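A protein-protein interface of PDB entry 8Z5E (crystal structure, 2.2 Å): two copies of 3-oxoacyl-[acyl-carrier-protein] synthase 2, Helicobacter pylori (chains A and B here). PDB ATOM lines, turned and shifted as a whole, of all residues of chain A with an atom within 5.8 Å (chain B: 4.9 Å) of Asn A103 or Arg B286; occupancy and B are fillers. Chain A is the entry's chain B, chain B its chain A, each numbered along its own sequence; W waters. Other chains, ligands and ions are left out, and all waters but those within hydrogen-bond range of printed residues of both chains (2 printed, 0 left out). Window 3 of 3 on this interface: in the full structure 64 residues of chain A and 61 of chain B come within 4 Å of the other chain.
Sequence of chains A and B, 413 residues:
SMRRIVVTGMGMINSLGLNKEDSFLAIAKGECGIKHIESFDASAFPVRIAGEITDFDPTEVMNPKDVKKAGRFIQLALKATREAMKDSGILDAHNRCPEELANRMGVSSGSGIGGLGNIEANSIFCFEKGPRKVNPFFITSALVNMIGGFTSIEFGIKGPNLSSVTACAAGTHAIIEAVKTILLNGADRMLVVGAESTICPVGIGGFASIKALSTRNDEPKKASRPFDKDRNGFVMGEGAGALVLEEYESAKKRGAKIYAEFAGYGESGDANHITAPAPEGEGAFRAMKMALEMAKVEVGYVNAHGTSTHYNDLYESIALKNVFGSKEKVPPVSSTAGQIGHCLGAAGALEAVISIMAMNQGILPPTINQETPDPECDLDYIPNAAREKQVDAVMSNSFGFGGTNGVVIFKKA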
ATOM      1  N   PRO A  98     -12.490  21.318 -12.393  1.00  0.00           N
ATOM      2  CA  PRO A  98     -11.696  20.420 -13.245  1.00  0.00           C
ATOM      3  C   PRO A  98     -11.279  21.124 -14.531  1.00  0.00           C
ATOM      4  O   PRO A  98     -12.026  21.933 -15.083  1.00  0.00           O
ATOM      5  CB  PRO A  98     -12.645  19.245 -13.523  1.00  0.00           C
ATOM      6  CG  PRO A  98     -13.644  19.263 -12.418  1.00  0.00           C
ATOM      7  CD  PRO A  98     -13.736  20.694 -11.905  1.00  0.00           C
ATOM      8  N   GLU A  99     -10.064  20.810 -14.997  1.00  0.00           N
ATOM      9  CA  GLU A  99      -9.484  21.549 -16.115  1.00  0.00           C
ATOM     10  C   GLU A  99     -10.305  21.386 -17.382  1.00  0.00           C
ATOM     11  O   GLU A  99     -10.480  22.341 -18.148  1.00  0.00           O
ATOM     12  CB  GLU A  99      -8.048  21.101 -16.370  1.00  0.00           C
ATOM     13  CG  GLU A  99      -7.260  20.732 -15.133  1.00  0.00           C
ATOM     14  CD  GLU A  99      -5.903  20.131 -15.484  1.00  0.00           C
ATOM     15  OE1 GLU A  99      -4.958  20.913 -15.754  1.00  0.00           O
ATOM     16  OE2 GLU A  99      -5.782  18.883 -15.487  1.00  0.00           O
ATOM     17  N   GLU A 100     -10.809  20.181 -17.628  1.00  0.00           N
ATOM     18  CA  GLU A 100     -11.588  19.926 -18.831  1.00  0.00           C
ATOM     19  C   GLU A 100     -12.946  20.614 -18.802  1.00  0.00           C
ATOM     20  O   GLU A 100     -13.620  20.656 -19.835  1.00  0.00           O
ATOM     21  CB  GLU A 100     -11.752  18.412 -19.022  1.00  0.00           C
ATOM     22  CG  GLU A 100     -12.878  17.784 -18.218  1.00  0.00           C
ATOM     23  CD  GLU A 100     -12.430  17.289 -16.857  1.00  0.00           C
ATOM     24  OE1 GLU A 100     -11.270  17.564 -16.469  1.00  0.00           O
ATOM     25  OE2 GLU A 100     -13.247  16.631 -16.170  1.00  0.00           O
ATOM     26  N   LEU A 101     -13.361  21.140 -17.650  1.00  0.00           N
ATOM     27  CA  LEU A 101     -14.593  21.906 -17.534  1.00  0.00           C
ATOM     28  C   LEU A 101     -14.361  23.403 -17.356  1.00  0.00           C
ATOM     29  O   LEU A 101     -15.329  24.170 -17.419  1.00  0.00           O
ATOM     30  CB  LEU A 101     -15.434  21.387 -16.352  1.00  0.00           C
ATOM     31  CG  LEU A 101     -15.857  19.913 -16.375  1.00  0.00           C
ATOM     32  CD1 LEU A 101     -16.984  19.636 -15.386  1.00  0.00           C
ATOM     33  CD2 LEU A 101     -16.267  19.495 -17.766  1.00  0.00           C
ATOM     34  N   ALA A 102     -13.109  23.832 -17.165  1.00  0.00           N
ATOM     35  CA  ALA A 102     -12.829  25.191 -16.717  1.00  0.00           C
ATOM     36  C   ALA A 102     -13.174  26.234 -17.776  1.00  0.00           C
ATOM     37  O   ALA A 102     -13.641  27.332 -17.438  1.00  0.00           O
ATOM     38  CB  ALA A 102     -11.358  25.310 -16.313  1.00  0.00           C
ATOM     39  N   ASN A 103     -12.934  25.925 -19.056  1.00  0.00           N
ATOM     40  CA  ASN A 103     -13.211  26.881 -20.121  1.00  0.00           C
ATOM     41  C   ASN A 103     -14.704  27.171 -20.280  1.00  0.00           C
ATOM     42  O   ASN A 103     -15.067  28.200 -20.860  1.00  0.00           O
ATOM     43  CB  ASN A 103     -12.650  26.370 -21.449  1.00  0.00           C
ATOM     44  CG  ASN A 103     -11.143  26.480 -21.524  1.00  0.00           C
ATOM     45  OD1 ASN A 103     -10.497  26.909 -20.577  1.00  0.00           O
ATOM     46  ND2 ASN A 103     -10.577  26.098 -22.657  1.00  0.00           N
ATOM     47  N   ARG A 104     -15.569  26.284 -19.798  1.00  0.00           N
ATOM     48  CA  ARG A 104     -16.998  26.362 -20.045  1.00  0.00           C
ATOM     49  C   ARG A 104     -17.760  26.737 -18.789  1.00  0.00           C
ATOM     50  O   ARG A 104     -18.988  26.643 -18.759  1.00  0.00           O
ATOM     51  CB  ARG A 104     -17.527  25.029 -20.596  1.00  0.00           C
ATOM     52  CG  ARG A 104     -17.080  24.724 -22.024  1.00  0.00           C
ATOM     53  CD  ARG A 104     -17.777  25.632 -22.994  1.00  0.00           C
ATOM     54  NE  ARG A 104     -19.214  25.370 -23.013  1.00  0.00           N
ATOM     55  CZ  ARG A 104     -20.088  26.035 -23.756  1.00  0.00           C
ATOM     56  NH1 ARG A 104     -19.712  27.038 -24.533  1.00  0.00           N
ATOM     57  NH2 ARG A 104     -21.367  25.665 -23.742  1.00  0.00           N
ATOM     58  N   MET A 105     -17.060  27.120 -17.740  1.00  0.00           N
ATOM     59  CA  MET A 105     -17.712  27.588 -16.538  1.00  0.00           C
ATOM     60  C   MET A 105     -17.212  28.988 -16.278  1.00  0.00           C
ATOM     61  O   MET A 105     -15.999  29.211 -16.172  1.00  0.00           O
ATOM     62  CB  MET A 105     -17.469  26.662 -15.345  1.00  0.00           C
ATOM     63  CG  MET A 105     -18.239  27.099 -14.117  1.00  0.00           C
ATOM     64  SD  MET A 105     -17.945  26.085 -12.659  1.00  0.00           S
ATOM     65  CE  MET A 105     -19.400  26.509 -11.699  1.00  0.00           C
ATOM     66  N   LYS A 158     -12.681  29.674 -16.178  1.00  0.00           N
ATOM     67  CA  LYS A 158     -12.143  30.484 -17.264  1.00  0.00           C
ATOM     68  C   LYS A 158     -13.187  30.847 -18.305  1.00  0.00           C
ATOM     69  O   LYS A 158     -12.821  31.383 -19.363  1.00  0.00           O
ATOM     70  CB  LYS A 158     -10.979  29.756 -17.945  1.00  0.00           C
ATOM     71  CG  LYS A 158      -9.894  29.298 -16.997  1.00  0.00           C
ATOM     72  CD  LYS A 158      -8.813  28.498 -17.718  1.00  0.00           C
ATOM     73  CE  LYS A 158      -7.444  28.842 -17.144  1.00  0.00           C
ATOM     74  NZ  LYS A 158      -6.373  27.918 -17.613  1.00  0.00           N
ATOM     75  N   GLY A 159     -14.467  30.568 -18.046  1.00  0.00           N
ATOM     76  CA  GLY A 159     -15.538  30.970 -18.927  1.00  0.00           C
ATOM     77  C   GLY A 159     -15.839  32.464 -18.859  1.00  0.00           C
ATOM     78  O   GLY A 159     -15.074  33.245 -18.273  1.00  0.00           O
ATOM     79  N   PRO A 160     -16.954  32.890 -19.463  1.00  0.00           N
ATOM     80  CA  PRO A 160     -17.308  34.317 -19.440  1.00  0.00           C
ATOM     81  C   PRO A 160     -17.288  34.866 -18.025  1.00  0.00           C
ATOM     82  O   PRO A 160     -17.801  34.251 -17.092  1.00  0.00           O
ATOM     83  CB  PRO A 160     -18.717  34.350 -20.050  1.00  0.00           C
ATOM     84  CG  PRO A 160     -18.738  33.121 -20.965  1.00  0.00           C
ATOM     85  CD  PRO A 160     -17.952  32.081 -20.181  1.00  0.00           C
ATOM     86  N   GLY A 186     -22.925  30.127 -24.405  1.00  0.00           N
ATOM     87  CA  GLY A 186     -21.630  30.684 -24.067  1.00  0.00           C
ATOM     88  C   GLY A 186     -20.956  30.019 -22.888  1.00  0.00           C
ATOM     89  O   GLY A 186     -19.787  30.302 -22.600  1.00  0.00           O
ATOM     90  N   SER B 268     -14.208  35.550 -22.089  1.00  0.00           N
ATOM     91  CA  SER B 268     -13.441  34.554 -21.369  1.00  0.00           C
ATOM     92  C   SER B 268     -12.861  35.242 -20.156  1.00  0.00           C
ATOM     93  O   SER B 268     -12.856  36.471 -20.070  1.00  0.00           O
ATOM     94  CB  SER B 268     -12.323  33.975 -22.240  1.00  0.00           C
ATOM     95  OG  SER B 268     -11.355  34.987 -22.508  1.00  0.00           O
ATOM     96  N   GLY B 269     -12.373  34.430 -19.222  1.00  0.00           N
ATOM     97  CA  GLY B 269     -11.536  34.919 -18.146  1.00  0.00           C
ATOM     98  C   GLY B 269     -10.216  34.172 -18.120  1.00  0.00           C
ATOM     99  O   GLY B 269     -10.143  32.991 -18.465  1.00  0.00           O
ATOM    100  N   ASP B 270      -9.163  34.888 -17.693  1.00  0.00           N
ATOM    101  CA  ASP B 270      -7.831  34.296 -17.559  1.00  0.00           C
ATOM    102  C   ASP B 270      -7.744  33.321 -16.382  1.00  0.00           C
ATOM    103  O   ASP B 270      -7.021  32.321 -16.457  1.00  0.00           O
ATOM    104  CB  ASP B 270      -6.777  35.393 -17.366  1.00  0.00           C
ATOM    105  CG  ASP B 270      -6.579  36.264 -18.594  1.00  0.00           C
ATOM    106  OD1 ASP B 270      -7.132  35.943 -19.671  1.00  0.00           O
ATOM    107  OD2 ASP B 270      -5.841  37.276 -18.464  1.00  0.00           O
ATOM    108  N   GLU B 282      -3.477  33.838 -23.189  1.00  0.00           N
ATOM    109  CA  GLU B 282      -4.301  32.655 -23.444  1.00  0.00           C
ATOM    110  C   GLU B 282      -5.797  32.969 -23.365  1.00  0.00           C
ATOM    111  O   GLU B 282      -6.588  32.465 -24.168  1.00  0.00           O
ATOM    112  CB  GLU B 282      -3.924  31.558 -22.442  1.00  0.00           C
ATOM    113  CG  GLU B 282      -4.589  30.228 -22.669  1.00  0.00           C
ATOM    114  CD  GLU B 282      -5.896  30.076 -21.899  1.00  0.00           C
ATOM    115  OE1 GLU B 282      -6.138  30.819 -20.909  1.00  0.00           O
ATOM    116  OE2 GLU B 282      -6.681  29.191 -22.289  1.00  0.00           O
ATOM    117  N   GLY B 283      -6.207  33.805 -22.409  1.00  0.00           N
ATOM    118  CA  GLY B 283      -7.612  34.172 -22.327  1.00  0.00           C
ATOM    119  C   GLY B 283      -8.054  35.030 -23.497  1.00  0.00           C
ATOM    120  O   GLY B 283      -9.151  34.843 -24.037  1.00  0.00           O
ATOM    121  N   ALA B 284      -7.207  35.985 -23.895  1.00  0.00           N
ATOM    122  CA  ALA B 284      -7.437  36.755 -25.113  1.00  0.00           C
ATOM    123  C   ALA B 284      -7.552  35.844 -26.323  1.00  0.00           C
ATOM    124  O   ALA B 284      -8.421  36.039 -27.184  1.00  0.00           O
ATOM    125  CB  ALA B 284      -6.298  37.755 -25.327  1.00  0.00           C
ATOM    126  N   PHE B 285      -6.662  34.856 -26.418  1.00  0.00           N
ATOM    127  CA  PHE B 285      -6.713  33.921 -27.540  1.00  0.00           C
ATOM    128  C   PHE B 285      -8.080  33.260 -27.612  1.00  0.00           C
ATOM    129  O   PHE B 285      -8.725  33.253 -28.662  1.00  0.00           O
ATOM    130  CB  PHE B 285      -5.595  32.873 -27.405  1.00  0.00           C
ATOM    131  CG  PHE B 285      -5.819  31.626 -28.221  1.00  0.00           C
ATOM    132  CD1 PHE B 285      -6.553  30.564 -27.708  1.00  0.00           C
ATOM    133  CD2 PHE B 285      -5.269  31.508 -29.494  1.00  0.00           C
ATOM    134  CE1 PHE B 285      -6.768  29.417 -28.462  1.00  0.00           C
ATOM    135  CE2 PHE B 285      -5.473  30.366 -30.257  1.00  0.00           C
ATOM    136  CZ  PHE B 285      -6.222  29.316 -29.740  1.00  0.00           C
ATOM    137  N   ARG B 286      -8.548  32.716 -26.486  1.00  0.00           N
ATOM    138  CA  ARG B 286      -9.832  32.020 -26.484  1.00  0.00           C
ATOM    139  C   ARG B 286     -10.995  32.956 -26.823  1.00  0.00           C
ATOM    140  O   ARG B 286     -11.897  32.580 -27.579  1.00  0.00           O
ATOM    141  CB  ARG B 286     -10.058  31.351 -25.135  1.00  0.00           C
ATOM    142  CG  ARG B 286      -9.204  30.110 -24.901  1.00  0.00           C
ATOM    143  CD  ARG B 286      -9.584  29.448 -23.577  1.00  0.00           C
ATOM    144  NE  ARG B 286      -9.009  30.169 -22.444  1.00  0.00           N
ATOM    145  CZ  ARG B 286      -9.717  30.730 -21.467  1.00  0.00           C
ATOM    146  NH1 ARG B 286     -11.039  30.646 -21.434  1.00  0.00           N
ATOM    147  NH2 ARG B 286      -9.080  31.399 -20.502  1.00  0.00           N
ATOM    148  N   ALA B 287     -10.996  34.185 -26.292  1.00  0.00           N
ATOM    149  CA  ALA B 287     -12.092  35.103 -26.620  1.00  0.00           C
ATOM    150  C   ALA B 287     -12.083  35.456 -28.104  1.00  0.00           C
ATOM    151  O   ALA B 287     -13.137  35.492 -28.757  1.00  0.00           O
ATOM    152  CB  ALA B 287     -12.010  36.366 -25.762  1.00  0.00           C
ATOM    153  N   MET B 288     -10.897  35.684 -28.660  1.00  0.00           N
ATOM    154  CA  MET B 288     -10.791  35.991 -30.082  1.00  0.00           C
ATOM    155  C   MET B 288     -11.221  34.793 -30.929  1.00  0.00           C
ATOM    156  O   MET B 288     -11.962  34.949 -31.906  1.00  0.00           O
ATOM    157  CB  MET B 288      -9.353  36.400 -30.394  1.00  0.00           C
ATOM    158  CG  MET B 288      -9.079  37.866 -30.203  1.00  0.00           C
ATOM    159  SD  MET B 288      -7.379  38.309 -30.652  1.00  0.00           S
ATOM    160  CE  MET B 288      -6.372  37.213 -29.629  1.00  0.00           C
ATOM    161  N   LYS B 289     -10.776  33.589 -30.550  1.00  0.00           N
ATOM    162  CA  LYS B 289     -11.156  32.382 -31.277  1.00  0.00           C
ATOM    163  C   LYS B 289     -12.668  32.188 -31.280  1.00  0.00           C
ATOM    164  O   LYS B 289     -13.258  31.852 -32.312  1.00  0.00           O
ATOM    165  CB  LYS B 289     -10.465  31.160 -30.668  1.00  0.00           C
ATOM    166  CG  LYS B 289     -10.853  29.832 -31.319  1.00  0.00           C
ATOM    167  CD  LYS B 289      -9.912  28.670 -30.941  1.00  0.00           C
ATOM    168  CE  LYS B 289     -10.119  28.162 -29.506  1.00  0.00           C
ATOM    169  NZ  LYS B 289     -11.381  27.366 -29.344  1.00  0.00           N
ATOM    170  N   MET B 290     -13.317  32.402 -30.138  1.00  0.00           N
ATOM    171  CA  MET B 290     -14.763  32.222 -30.107  1.00  0.00           C
ATOM    172  C   MET B 290     -15.458  33.245 -30.988  1.00  0.00           C
ATOM    173  O   MET B 290     -16.361  32.898 -31.756  1.00  0.00           O
ATOM    174  CB  MET B 290     -15.291  32.287 -28.675  1.00  0.00           C
ATOM    175  CG  MET B 290     -15.361  30.892 -28.071  1.00  0.00           C
ATOM    176  SD  MET B 290     -15.468  30.769 -26.271  1.00  0.00           S
ATOM    177  CE  MET B 290     -14.307  31.999 -25.678  1.00  0.00           C
HETATM  178  O   HOH W   1     -17.803  31.152 -23.969  1.00  0.00           O
HETATM  179  O   HOH W   2     -13.283  29.612 -23.123  1.00  0.00           O
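Among the printed residues, 7 pairs touch across the chains.
No position is printed for both chains. Of the 7 pairs that touch across the chains among the printed residues, none has its exchanged pair printed and touching as well.
Asn A103 touches just one residue of chain B: Arg B286. Of the printed residues of chain B, Lys A158 touches Ser B268 (3.8 Å), Gly B269 (3.1 Å), Asp B270 (3.6 Å) and Arg B286 (2.8 Å). Of the printed residues of chain B, Gly A159 touches Ser B268 and Gly B269. Arg B286 touches two residues of chain A.
Among the printed residues, pairs that only touch across the chains: Gly A159 with Ser B268 (3.5 Å), Lys A158 with Asp B270 (3.6 Å), Asn A103 with Arg B286 (3.6 Å) and Lys A158 with Ser B268 (3.8 Å).
The backbone NH of Gly B269 lies within hydrogen-bond range of the backbone carbonyl oxygen of Lys A158. The backbone carbonyl oxygen (O) of Gly A159 lies within hydrogen-bond range of the backbone NH (N) of Gly B269. The guanidinium group (NH1) of Arg B286 sits at hydrogen-bond distance from the backbone carbonyl oxygen (O) of Lys A158, 2.8 Å away.
The side-chain hydroxyl of Ser B268 lies within hydrogen-bond range of the backbone carbonyl oxygen of Gly B283, 2.7 Å away. NH2 of Arg B286 lies within hydrogen-bond range of O of Gly B269 (2.8 Å). The guanidinium group of Arg B286 is in salt-bridge range of the side-chain carboxylate of Glu B282 (2.5 Å). The backbone NH of Lys A158 lies within hydrogen-bond range of the backbone carbonyl oxygen of Ala A102 (2.8 Å). The backbone NH (N) of Gly A159 sits at hydrogen-bond distance from the backbone carbonyl oxygen (O) of Ala A102, 3.4 Å away. O of Met A105 lies within hydrogen-bond range of N of Gly A159, at 2.8 Å.
Water W1 lies within hydrogen-bond range of the backbone carbonyl oxygen of Gly A186 and the side-chain sulfur of Met B290. Water W2 lies within hydrogen-bond range of NH1 of Arg B286 (3.0 Å) and O of Asn A103 (3.2 Å).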
